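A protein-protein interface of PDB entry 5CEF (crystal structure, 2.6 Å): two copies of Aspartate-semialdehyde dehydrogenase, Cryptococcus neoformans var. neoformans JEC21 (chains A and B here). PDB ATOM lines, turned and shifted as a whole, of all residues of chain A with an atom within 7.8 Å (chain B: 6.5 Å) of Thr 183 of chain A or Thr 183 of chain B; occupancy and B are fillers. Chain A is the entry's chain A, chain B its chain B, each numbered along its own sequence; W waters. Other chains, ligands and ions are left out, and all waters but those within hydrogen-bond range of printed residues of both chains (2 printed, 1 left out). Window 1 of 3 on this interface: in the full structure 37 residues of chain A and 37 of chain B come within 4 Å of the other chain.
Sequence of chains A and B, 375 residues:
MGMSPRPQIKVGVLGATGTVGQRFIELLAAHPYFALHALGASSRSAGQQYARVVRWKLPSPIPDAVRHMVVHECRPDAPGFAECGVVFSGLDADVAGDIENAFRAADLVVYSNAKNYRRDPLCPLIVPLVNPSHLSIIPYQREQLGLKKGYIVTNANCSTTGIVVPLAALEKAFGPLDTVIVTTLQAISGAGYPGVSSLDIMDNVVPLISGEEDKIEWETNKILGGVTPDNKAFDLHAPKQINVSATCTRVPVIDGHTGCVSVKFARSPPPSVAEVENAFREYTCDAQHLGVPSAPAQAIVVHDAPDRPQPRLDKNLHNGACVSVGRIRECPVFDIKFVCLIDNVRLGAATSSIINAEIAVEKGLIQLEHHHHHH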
ATOM      1  N   ILE A 163     -20.647 -15.865   9.471  1.00  0.00           N
ATOM      2  CA  ILE A 163     -19.823 -15.998  10.651  1.00  0.00           C
ATOM      3  C   ILE A 163     -18.449 -15.326  10.516  1.00  0.00           C
ATOM      4  O   ILE A 163     -18.047 -14.543  11.386  1.00  0.00           O
ATOM      5  CB  ILE A 163     -19.639 -17.474  10.990  1.00  0.00           C
ATOM      6  CG1 ILE A 163     -20.964 -18.021  11.458  1.00  0.00           C
ATOM      7  CG2 ILE A 163     -18.621 -17.669  12.096  1.00  0.00           C
ATOM      8  CD1 ILE A 163     -21.058 -19.503  11.234  1.00  0.00           C
ATOM      9  N   VAL A 180     -13.711 -20.453  18.978  1.00  0.00           N
ATOM     10  CA  VAL A 180     -15.036 -20.055  18.524  1.00  0.00           C
ATOM     11  C   VAL A 180     -16.048 -21.193  18.565  1.00  0.00           C
ATOM     12  O   VAL A 180     -15.800 -22.272  18.029  1.00  0.00           O
ATOM     13  CB  VAL A 180     -15.001 -19.541  17.075  1.00  0.00           C
ATOM     14  CG1 VAL A 180     -16.417 -19.186  16.608  1.00  0.00           C
ATOM     15  CG2 VAL A 180     -14.096 -18.318  16.932  1.00  0.00           C
ATOM     16  N   ILE A 181     -17.197 -20.940  19.178  1.00  0.00           N
ATOM     17  CA  ILE A 181     -18.307 -21.896  19.192  1.00  0.00           C
ATOM     18  C   ILE A 181     -19.498 -21.232  18.584  1.00  0.00           C
ATOM     19  O   ILE A 181     -19.766 -20.061  18.851  1.00  0.00           O
ATOM     20  CB  ILE A 181     -18.642 -22.392  20.611  1.00  0.00           C
ATOM     21  CG1 ILE A 181     -17.504 -23.294  21.086  1.00  0.00           C
ATOM     22  CG2 ILE A 181     -19.939 -23.172  20.634  1.00  0.00           C
ATOM     23  CD1 ILE A 181     -17.882 -24.289  22.145  1.00  0.00           C
ATOM     24  N   VAL A 182     -20.187 -21.949  17.722  1.00  0.00           N
ATOM     25  CA  VAL A 182     -21.265 -21.342  17.007  1.00  0.00           C
ATOM     26  C   VAL A 182     -22.414 -22.316  16.755  1.00  0.00           C
ATOM     27  O   VAL A 182     -22.187 -23.455  16.350  1.00  0.00           O
ATOM     28  CB  VAL A 182     -20.783 -20.750  15.669  1.00  0.00           C
ATOM     29  CG1 VAL A 182     -20.116 -21.802  14.789  1.00  0.00           C
ATOM     30  CG2 VAL A 182     -21.959 -20.113  14.914  1.00  0.00           C
ATOM     31  N   THR A 183     -23.641 -21.851  16.964  1.00  0.00           N
ATOM     32  CA  THR A 183     -24.799 -22.569  16.518  1.00  0.00           C
ATOM     33  C   THR A 183     -25.475 -21.707  15.434  1.00  0.00           C
ATOM     34  O   THR A 183     -25.721 -20.539  15.663  1.00  0.00           O
ATOM     35  CB  THR A 183     -25.773 -22.844  17.692  1.00  0.00           C
ATOM     36  OG1 THR A 183     -25.149 -23.669  18.684  1.00  0.00           O
ATOM     37  CG2 THR A 183     -27.010 -23.567  17.192  1.00  0.00           C
ATOM     38  N   THR A 184     -25.811 -22.292  14.287  1.00  0.00           N
ATOM     39  CA  THR A 184     -26.545 -21.561  13.273  1.00  0.00           C
ATOM     40  C   THR A 184     -28.010 -21.977  13.205  1.00  0.00           C
ATOM     41  O   THR A 184     -28.380 -23.124  13.513  1.00  0.00           O
ATOM     42  CB  THR A 184     -25.959 -21.721  11.855  1.00  0.00           C
ATOM     43  OG1 THR A 184     -26.111 -23.069  11.422  1.00  0.00           O
ATOM     44  CG2 THR A 184     -24.514 -21.351  11.834  1.00  0.00           C
ATOM     45  N   LEU A 185     -28.834 -20.999  12.809  1.00  0.00           N
ATOM     46  CA  LEU A 185     -30.228 -21.199  12.507  1.00  0.00           C
ATOM     47  C   LEU A 185     -30.421 -20.704  11.082  1.00  0.00           C
ATOM     48  O   LEU A 185     -30.557 -19.505  10.827  1.00  0.00           O
ATOM     49  CB  LEU A 185     -31.112 -20.427  13.473  1.00  0.00           C
ATOM     50  CG  LEU A 185     -31.218 -20.893  14.918  1.00  0.00           C
ATOM     51  CD1 LEU A 185     -29.903 -20.735  15.635  1.00  0.00           C
ATOM     52  CD2 LEU A 185     -32.268 -20.090  15.674  1.00  0.00           C
ATOM     53  N   GLN A 186     -30.441 -21.634  10.138  1.00  0.00           N
ATOM     54  CA  GLN A 186     -30.376 -21.287   8.744  1.00  0.00           C
ATOM     55  C   GLN A 186     -31.749 -21.330   8.107  1.00  0.00           C
ATOM     56  O   GLN A 186     -32.517 -22.221   8.334  1.00  0.00           O
ATOM     57  CB  GLN A 186     -29.319 -22.172   8.038  1.00  0.00           C
ATOM     58  CG  GLN A 186     -27.946 -22.004   8.713  1.00  0.00           C
ATOM     59  CD  GLN A 186     -26.813 -22.835   8.127  1.00  0.00           C
ATOM     60  OE1 GLN A 186     -25.897 -23.248   8.856  1.00  0.00           O
ATOM     61  NE2 GLN A 186     -26.843 -23.051   6.837  1.00  0.00           N
ATOM     62  N   ILE A 216     -17.653 -24.950   7.961  1.00  0.00           N
ATOM     63  CA  ILE A 216     -17.365 -23.870   8.869  1.00  0.00           C
ATOM     64  C   ILE A 216     -16.103 -24.123   9.679  1.00  0.00           C
ATOM     65  O   ILE A 216     -15.305 -23.226   9.856  1.00  0.00           O
ATOM     66  CB  ILE A 216     -18.558 -23.547   9.828  1.00  0.00           C
ATOM     67  CG1 ILE A 216     -19.724 -22.925   9.048  1.00  0.00           C
ATOM     68  CG2 ILE A 216     -18.169 -22.531  10.892  1.00  0.00           C
ATOM     69  CD1 ILE A 216     -21.061 -22.935   9.781  1.00  0.00           C
ATOM     70  N   SER A 245     -15.962 -24.964  16.738  1.00  0.00           N
ATOM     71  CA  SER A 245     -16.951 -26.034  16.847  1.00  0.00           C
ATOM     72  C   SER A 245     -18.305 -25.471  16.500  1.00  0.00           C
ATOM     73  O   SER A 245     -18.760 -24.517  17.132  1.00  0.00           O
ATOM     74  CB  SER A 245     -16.958 -26.596  18.264  1.00  0.00           C
ATOM     75  OG  SER A 245     -17.852 -27.658  18.422  1.00  0.00           O
ATOM     76  N   ALA A 246     -18.950 -26.099  15.528  1.00  0.00           N
ATOM     77  CA  ALA A 246     -20.239 -25.660  15.037  1.00  0.00           C
ATOM     78  C   ALA A 246     -21.360 -26.718  15.126  1.00  0.00           C
ATOM     79  O   ALA A 246     -21.122 -27.921  15.008  1.00  0.00           O
ATOM     80  CB  ALA A 246     -20.091 -25.250  13.587  1.00  0.00           C
ATOM     81  N   THR A 247     -22.587 -26.238  15.297  1.00  0.00           N
ATOM     82  CA  THR A 247     -23.769 -27.031  15.076  1.00  0.00           C
ATOM     83  C   THR A 247     -24.635 -26.202  14.142  1.00  0.00           C
ATOM     84  O   THR A 247     -24.815 -25.010  14.378  1.00  0.00           O
ATOM     85  CB  THR A 247     -24.517 -27.263  16.378  1.00  0.00           C
ATOM     86  OG1 THR A 247     -23.653 -27.803  17.388  1.00  0.00           O
ATOM     87  CG2 THR A 247     -25.620 -28.216  16.144  1.00  0.00           C
ATOM     88  N   CYS A 248     -25.127 -26.804  13.061  1.00  0.00           N
ATOM     89  CA  CYS A 248     -25.853 -26.070  12.032  1.00  0.00           C
ATOM     90  C   CYS A 248     -27.233 -26.629  11.911  1.00  0.00           C
ATOM     91  O   CYS A 248     -27.417 -27.846  11.766  1.00  0.00           O
ATOM     92  CB  CYS A 248     -25.155 -26.192  10.698  1.00  0.00           C
ATOM     93  SG  CYS A 248     -23.573 -25.321  10.657  1.00  0.00           S
ATOM     94  N   THR A 249     -28.239 -25.767  12.058  1.00  0.00           N
ATOM     95  CA  THR A 249     -29.618 -26.227  12.019  1.00  0.00           C
ATOM     96  C   THR A 249     -30.363 -25.492  10.949  1.00  0.00           C
ATOM     97  O   THR A 249     -29.958 -24.410  10.538  1.00  0.00           O
ATOM     98  CB  THR A 249     -30.338 -25.994  13.331  1.00  0.00           C
ATOM     99  OG1 THR A 249     -30.596 -24.602  13.469  1.00  0.00           O
ATOM    100  CG2 THR A 249     -29.517 -26.454  14.468  1.00  0.00           C
ATOM    101  N   THR A 258     -29.125 -16.904  10.836  1.00  0.00           N
ATOM    102  CA  THR A 258     -28.782 -16.361  12.137  1.00  0.00           C
ATOM    103  C   THR A 258     -27.718 -17.222  12.796  1.00  0.00           C
ATOM    104  O   THR A 258     -27.736 -18.434  12.649  1.00  0.00           O
ATOM    105  CB  THR A 258     -30.031 -16.345  13.003  1.00  0.00           C
ATOM    106  OG1 THR A 258     -31.041 -15.555  12.344  1.00  0.00           O
ATOM    107  CG2 THR A 258     -29.732 -15.792  14.351  1.00  0.00           C
ATOM    108  N   GLY A 259     -26.757 -16.600  13.478  1.00  0.00           N
ATOM    109  CA  GLY A 259     -25.683 -17.332  14.162  1.00  0.00           C
ATOM    110  C   GLY A 259     -25.522 -16.878  15.598  1.00  0.00           C
ATOM    111  O   GLY A 259     -25.573 -15.682  15.865  1.00  0.00           O
ATOM    112  N   CYS A 260     -25.338 -17.826  16.497  1.00  0.00           N
ATOM    113  CA  CYS A 260     -25.145 -17.552  17.907  1.00  0.00           C
ATOM    114  C   CYS A 260     -23.704 -17.944  18.264  1.00  0.00           C
ATOM    115  O   CYS A 260     -23.377 -19.109  18.293  1.00  0.00           O
ATOM    116  CB  CYS A 260     -26.134 -18.384  18.736  1.00  0.00           C
ATOM    117  SG  CYS A 260     -27.901 -17.987  18.507  1.00  0.00           S
ATOM    118  N   VAL A 261     -22.852 -16.954  18.512  1.00  0.00           N
ATOM    119  CA  VAL A 261     -21.420 -17.122  18.492  1.00  0.00           C
ATOM    120  C   VAL A 261     -20.805 -16.773  19.834  1.00  0.00           C
ATOM    121  O   VAL A 261     -21.134 -15.739  20.412  1.00  0.00           O
ATOM    122  CB  VAL A 261     -20.789 -16.236  17.394  1.00  0.00           C
ATOM    123  CG1 VAL A 261     -19.288 -16.480  17.259  1.00  0.00           C
ATOM    124  CG2 VAL A 261     -21.430 -16.526  16.045  1.00  0.00           C
ATOM    125  N   SER A 262     -19.916 -17.628  20.330  1.00  0.00           N
ATOM    126  CA  SER A 262     -19.073 -17.275  21.493  1.00  0.00           C
ATOM    127  C   SER A 262     -17.596 -17.266  21.088  1.00  0.00           C
ATOM    128  O   SER A 262     -17.151 -18.131  20.361  1.00  0.00           O
ATOM    129  CB  SER A 262     -19.285 -18.247  22.646  1.00  0.00           C
ATOM    130  OG  SER A 262     -20.666 -18.282  23.025  1.00  0.00           O
ATOM    131  N   PHE A 338     -22.376 -13.174  20.995  1.00  0.00           N
ATOM    132  CA  PHE A 338     -23.247 -12.302  20.220  1.00  0.00           C
ATOM    133  C   PHE A 338     -24.099 -13.086  19.254  1.00  0.00           C
ATOM    134  O   PHE A 338     -23.958 -14.297  19.112  1.00  0.00           O
ATOM    135  CB  PHE A 338     -22.420 -11.241  19.462  1.00  0.00           C
ATOM    136  CG  PHE A 338     -21.447 -11.809  18.471  1.00  0.00           C
ATOM    137  CD1 PHE A 338     -21.801 -11.998  17.185  1.00  0.00           C
ATOM    138  CD2 PHE A 338     -20.168 -12.108  18.827  1.00  0.00           C
ATOM    139  CE1 PHE A 338     -20.915 -12.504  16.253  1.00  0.00           C
ATOM    140  CE2 PHE A 338     -19.259 -12.588  17.898  1.00  0.00           C
ATOM    141  CZ  PHE A 338     -19.645 -12.810  16.606  1.00  0.00           C
ATOM    142  N   CYS A 340     -25.416 -12.933  15.147  1.00  0.00           N
ATOM    143  CA  CYS A 340     -25.170 -12.336  13.843  1.00  0.00           C
ATOM    144  C   CYS A 340     -26.219 -12.784  12.842  1.00  0.00           C
ATOM    145  O   CYS A 340     -26.855 -13.815  13.019  1.00  0.00           O
ATOM    146  CB  CYS A 340     -23.761 -12.714  13.332  1.00  0.00           C
ATOM    147  SG  CYS A 340     -23.380 -14.470  13.144  1.00  0.00           S
ATOM    148  N   ILE B 181     -21.594 -25.207  27.028  1.00  0.00           N
ATOM    149  CA  ILE B 181     -22.094 -24.161  26.182  1.00  0.00           C
ATOM    150  C   ILE B 181     -23.365 -24.667  25.494  1.00  0.00           C
ATOM    151  O   ILE B 181     -23.390 -25.768  24.980  1.00  0.00           O
ATOM    152  CB  ILE B 181     -21.026 -23.715  25.152  1.00  0.00           C
ATOM    153  CG1 ILE B 181     -19.917 -22.980  25.901  1.00  0.00           C
ATOM    154  CG2 ILE B 181     -21.634 -22.781  24.101  1.00  0.00           C
ATOM    155  CD1 ILE B 181     -19.123 -21.997  25.066  1.00  0.00           C
ATOM    156  N   VAL B 182     -24.395 -23.829  25.459  1.00  0.00           N
ATOM    157  CA  VAL B 182     -25.653 -24.234  24.866  1.00  0.00           C
ATOM    158  C   VAL B 182     -26.378 -23.115  24.094  1.00  0.00           C
ATOM    159  O   VAL B 182     -26.428 -22.001  24.552  1.00  0.00           O
ATOM    160  CB  VAL B 182     -26.570 -24.811  25.929  1.00  0.00           C
ATOM    161  CG1 VAL B 182     -26.806 -23.802  27.014  1.00  0.00           C
ATOM    162  CG2 VAL B 182     -27.867 -25.264  25.301  1.00  0.00           C
ATOM    163  N   THR B 183     -26.872 -23.426  22.895  1.00  0.00           N
ATOM    164  CA  THR B 183     -27.796 -22.553  22.186  1.00  0.00           C
ATOM    165  C   THR B 183     -29.165 -23.269  22.130  1.00  0.00           C
ATOM    166  O   THR B 183     -29.216 -24.450  21.757  1.00  0.00           O
ATOM    167  CB  THR B 183     -27.338 -22.260  20.757  1.00  0.00           C
ATOM    168  OG1 THR B 183     -26.081 -21.565  20.789  1.00  0.00           O
ATOM    169  CG2 THR B 183     -28.339 -21.413  20.072  1.00  0.00           C
ATOM    170  N   THR B 184     -30.245 -22.595  22.544  1.00  0.00           N
ATOM    171  CA  THR B 184     -31.559 -23.202  22.462  1.00  0.00           C
ATOM    172  C   THR B 184     -32.368 -22.614  21.306  1.00  0.00           C
ATOM    173  O   THR B 184     -32.186 -21.450  20.906  1.00  0.00           O
ATOM    174  CB  THR B 184     -32.385 -23.034  23.734  1.00  0.00           C
ATOM    175  OG1 THR B 184     -32.667 -21.649  23.933  1.00  0.00           O
ATOM    176  CG2 THR B 184     -31.650 -23.577  24.931  1.00  0.00           C
ATOM    177  N   LEU B 185     -33.246 -23.464  20.774  1.00  0.00           N
ATOM    178  CA  LEU B 185     -34.236 -23.078  19.805  1.00  0.00           C
ATOM    179  C   LEU B 185     -35.599 -23.465  20.417  1.00  0.00           C
ATOM    180  O   LEU B 185     -35.996 -24.630  20.373  1.00  0.00           O
ATOM    181  CB  LEU B 185     -34.011 -23.817  18.488  1.00  0.00           C
ATOM    182  CG  LEU B 185     -32.810 -23.433  17.639  1.00  0.00           C
ATOM    183  CD1 LEU B 185     -31.506 -23.782  18.299  1.00  0.00           C
ATOM    184  CD2 LEU B 185     -32.871 -24.134  16.308  1.00  0.00           C
ATOM    185  N   SER B 245     -22.588 -21.219  29.680  1.00  0.00           N
ATOM    186  CA  SER B 245     -22.908 -20.049  28.861  1.00  0.00           C
ATOM    187  C   SER B 245     -23.978 -20.429  27.874  1.00  0.00           C
ATOM    188  O   SER B 245     -23.798 -21.375  27.087  1.00  0.00           O
ATOM    189  CB  SER B 245     -21.681 -19.555  28.116  1.00  0.00           C
ATOM    190  OG  SER B 245     -21.947 -18.366  27.391  1.00  0.00           O
ATOM    191  N   ALA B 246     -25.080 -19.684  27.901  1.00  0.00           N
ATOM    192  CA  ALA B 246     -26.244 -19.954  27.046  1.00  0.00           C
ATOM    193  C   ALA B 246     -26.652 -18.793  26.135  1.00  0.00           C
ATOM    194  O   ALA B 246     -26.462 -17.635  26.455  1.00  0.00           O
ATOM    195  CB  ALA B 246     -27.414 -20.308  27.915  1.00  0.00           C
ATOM    196  N   THR B 247     -27.201 -19.122  24.985  1.00  0.00           N
ATOM    197  CA  THR B 247     -27.924 -18.172  24.175  1.00  0.00           C
ATOM    198  C   THR B 247     -29.256 -18.852  23.950  1.00  0.00           C
ATOM    199  O   THR B 247     -29.299 -20.018  23.521  1.00  0.00           O
ATOM    200  CB  THR B 247     -27.238 -17.928  22.809  1.00  0.00           C
ATOM    201  OG1 THR B 247     -25.874 -17.549  22.993  1.00  0.00           O
ATOM    202  CG2 THR B 247     -27.931 -16.839  22.078  1.00  0.00           C
ATOM    203  N   CYS B 248     -30.343 -18.142  24.177  1.00  0.00           N
ATOM    204  CA  CYS B 248     -31.667 -18.736  24.018  1.00  0.00           C
ATOM    205  C   CYS B 248     -32.420 -18.000  22.924  1.00  0.00           C
ATOM    206  O   CYS B 248     -32.534 -16.769  22.949  1.00  0.00           O
ATOM    207  CB  CYS B 248     -32.399 -18.629  25.324  1.00  0.00           C
ATOM    208  SG  CYS B 248     -31.675 -19.664  26.599  1.00  0.00           S
ATOM    209  N   THR B 249     -32.990 -18.745  21.994  1.00  0.00           N
ATOM    210  CA  THR B 249     -33.756 -18.155  20.920  1.00  0.00           C
ATOM    211  C   THR B 249     -35.130 -18.749  20.832  1.00  0.00           C
ATOM    212  O   THR B 249     -35.364 -19.810  21.325  1.00  0.00           O
ATOM    213  CB  THR B 249     -33.090 -18.384  19.563  1.00  0.00           C
ATOM    214  OG1 THR B 249     -33.242 -19.740  19.181  1.00  0.00           O
ATOM    215  CG2 THR B 249     -31.627 -18.083  19.638  1.00  0.00           C
ATOM    216  N   THR B 258     -35.472 -27.390  21.378  1.00  0.00           N
ATOM    217  CA  THR B 258     -34.263 -28.037  20.901  1.00  0.00           C
ATOM    218  C   THR B 258     -33.033 -27.340  21.475  1.00  0.00           C
ATOM    219  O   THR B 258     -33.031 -26.126  21.599  1.00  0.00           O
ATOM    220  CB  THR B 258     -34.240 -27.961  19.374  1.00  0.00           C
ATOM    221  OG1 THR B 258     -35.423 -28.581  18.853  1.00  0.00           O
ATOM    222  CG2 THR B 258     -33.004 -28.621  18.831  1.00  0.00           C
ATOM    223  N   GLY B 259     -32.032 -28.110  21.885  1.00  0.00           N
ATOM    224  CA  GLY B 259     -30.798 -27.559  22.445  1.00  0.00           C
ATOM    225  C   GLY B 259     -29.558 -28.104  21.749  1.00  0.00           C
ATOM    226  O   GLY B 259     -29.492 -29.291  21.473  1.00  0.00           O
ATOM    227  N   CYS B 260     -28.604 -27.224  21.436  1.00  0.00           N
ATOM    228  CA  CYS B 260     -27.351 -27.603  20.822  1.00  0.00           C
ATOM    229  C   CYS B 260     -26.228 -27.398  21.856  1.00  0.00           C
ATOM    230  O   CYS B 260     -25.907 -26.277  22.203  1.00  0.00           O
ATOM    231  CB  CYS B 260     -27.116 -26.749  19.577  1.00  0.00           C
ATOM    232  SG  CYS B 260     -28.381 -26.937  18.272  1.00  0.00           S
ATOM    233  N   VAL B 261     -25.656 -28.493  22.354  1.00  0.00           N
ATOM    234  CA  VAL B 261     -24.886 -28.480  23.585  1.00  0.00           C
ATOM    235  C   VAL B 261     -23.464 -28.979  23.363  1.00  0.00           C
ATOM    236  O   VAL B 261     -23.268 -30.010  22.696  1.00  0.00           O
ATOM    237  CB  VAL B 261     -25.566 -29.379  24.659  1.00  0.00           C
ATOM    238  CG1 VAL B 261     -24.819 -29.292  25.999  1.00  0.00           C
ATOM    239  CG2 VAL B 261     -27.007 -28.949  24.880  1.00  0.00           C
HETATM  240  O   HOH W   1     -25.045 -15.188  21.669  1.00  0.00           O
HETATM  241  O   HOH W   2     -23.635 -22.844  20.706  1.00  0.00           O
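The side-chain hydroxyl (OG1) of Thr 183 of chain B sits at hydrogen-bond distance from the side-chain hydroxyl (OG1) of Thr 183 of chain A, at 3.1 Å.
O of Ile 181 of chain A lies within hydrogen-bond range of N of Ser 262 of chain A (2.9 Å).
N of Thr 247 of chain A lies within hydrogen-bond range of O of Val 182 of chain A.
OG1 of Thr 249 of chain A is in hydrogen-bond range of O of Thr 184 of chain A, 2.7 Å away.
N of Leu 185 of chain A lies within hydrogen-bond range of O of Thr 258 of chain A (2.8 Å).
O of Val 182 of chain B is in hydrogen-bond range of N of Thr 247 of chain B.
The backbone carbonyl oxygen of Thr 183 of chain B lies within hydrogen-bond range of the backbone NH of Cys 260 of chain B (2.9 Å).
Among the printed residues, pairs that only touch across the chains: Ile 181 of chain A with Ile 181 of chain B (3.9 Å), Thr 183 of chain A with Cys 260 of chain B (3.8 Å), Leu 185 of chain A with Leu 185 of chain B (3.9 Å), Leu 185 of chain A with Thr 249 of chain B (3.7 Å), Thr 247 of chain A with Cys 260 of chain B (3.7 Å), Thr 249 of chain A with Leu 185 of chain B (3.7 Å), Thr 249 of chain A with Cys 260 of chain B (3.999 Å), Cys 260 of chain A with Thr 183 of chain B (3.8 Å), Cys 260 of chain A with Thr 247 of chain B (3.8 Å) and Cys 260 of chain A with Thr 249 of chain B (3.9 Å).
Of the printed residues of chain B, Ile 181 of chain A touches Ile 181.
Of chain B, only Thr 183 and Cys 260 come within 4 Å of Thr 183 of chain A.
Printed residues of chain B within 4 Å of Leu 185 of chain A: Leu 185 and Thr 249.
Printed residues of chain B within 4 Å of Cys 260 of chain A: Thr 183 (3.8 Å), Thr 247 (3.8 Å) and Thr 249 (3.9 Å).
Printed residues of chain A within 4 Å of Thr 183 of chain B: Thr 183 (3.1 Å) and Cys 260 (3.8 Å).
Of the printed residues of chain A, Leu 185 of chain B touches Leu 185 (3.9 Å) and Thr 249 (3.7 Å).
Of the printed residues of chain A, Thr 247 of chain B touches Cys 260 (3.8 Å).
Hydrophobic or aromatic side chains of chain B within 4 Å of the printed part of chain A: Ile 181 and Leu 185.
Printed residues of chain A that touch a printed residue of chain B: Ile 181, Thr 183, Leu 185, Thr 247, Thr 249 and Cys 260.
Along chain A the printed residues that touch a printed residue of chain B span positions 181 to 260.
Thr 183 of chain A touches Cys 260 of chain B, and with the chains exchanged Cys 260 of chain A touches Thr 183 of chain B.
Leu 185 of chain A touches its own counterpart, Leu 185 of chain B.
Leu 185 of chain A touches Thr 249 of chain B, and with the chains exchanged Thr 249 of chain A touches Leu 185 of chain B.
Thr 247 of chain A touches Cys 260 of chain B, and with the chains exchanged Cys 260 of chain A touches Thr 247 of chain B.
Of the 11 pairs that touch across the chains among the printed residues, 11 have their exchanged pair printed and touching as well.
Water W2 bridges OG1 of Thr 183 of chain A and OG1 of Thr 183 of chain B.
Water W1 bridges OG1 of Thr 247 of chain B (2.8 Å) and O of Phe 338 of chain A (2.9 Å).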
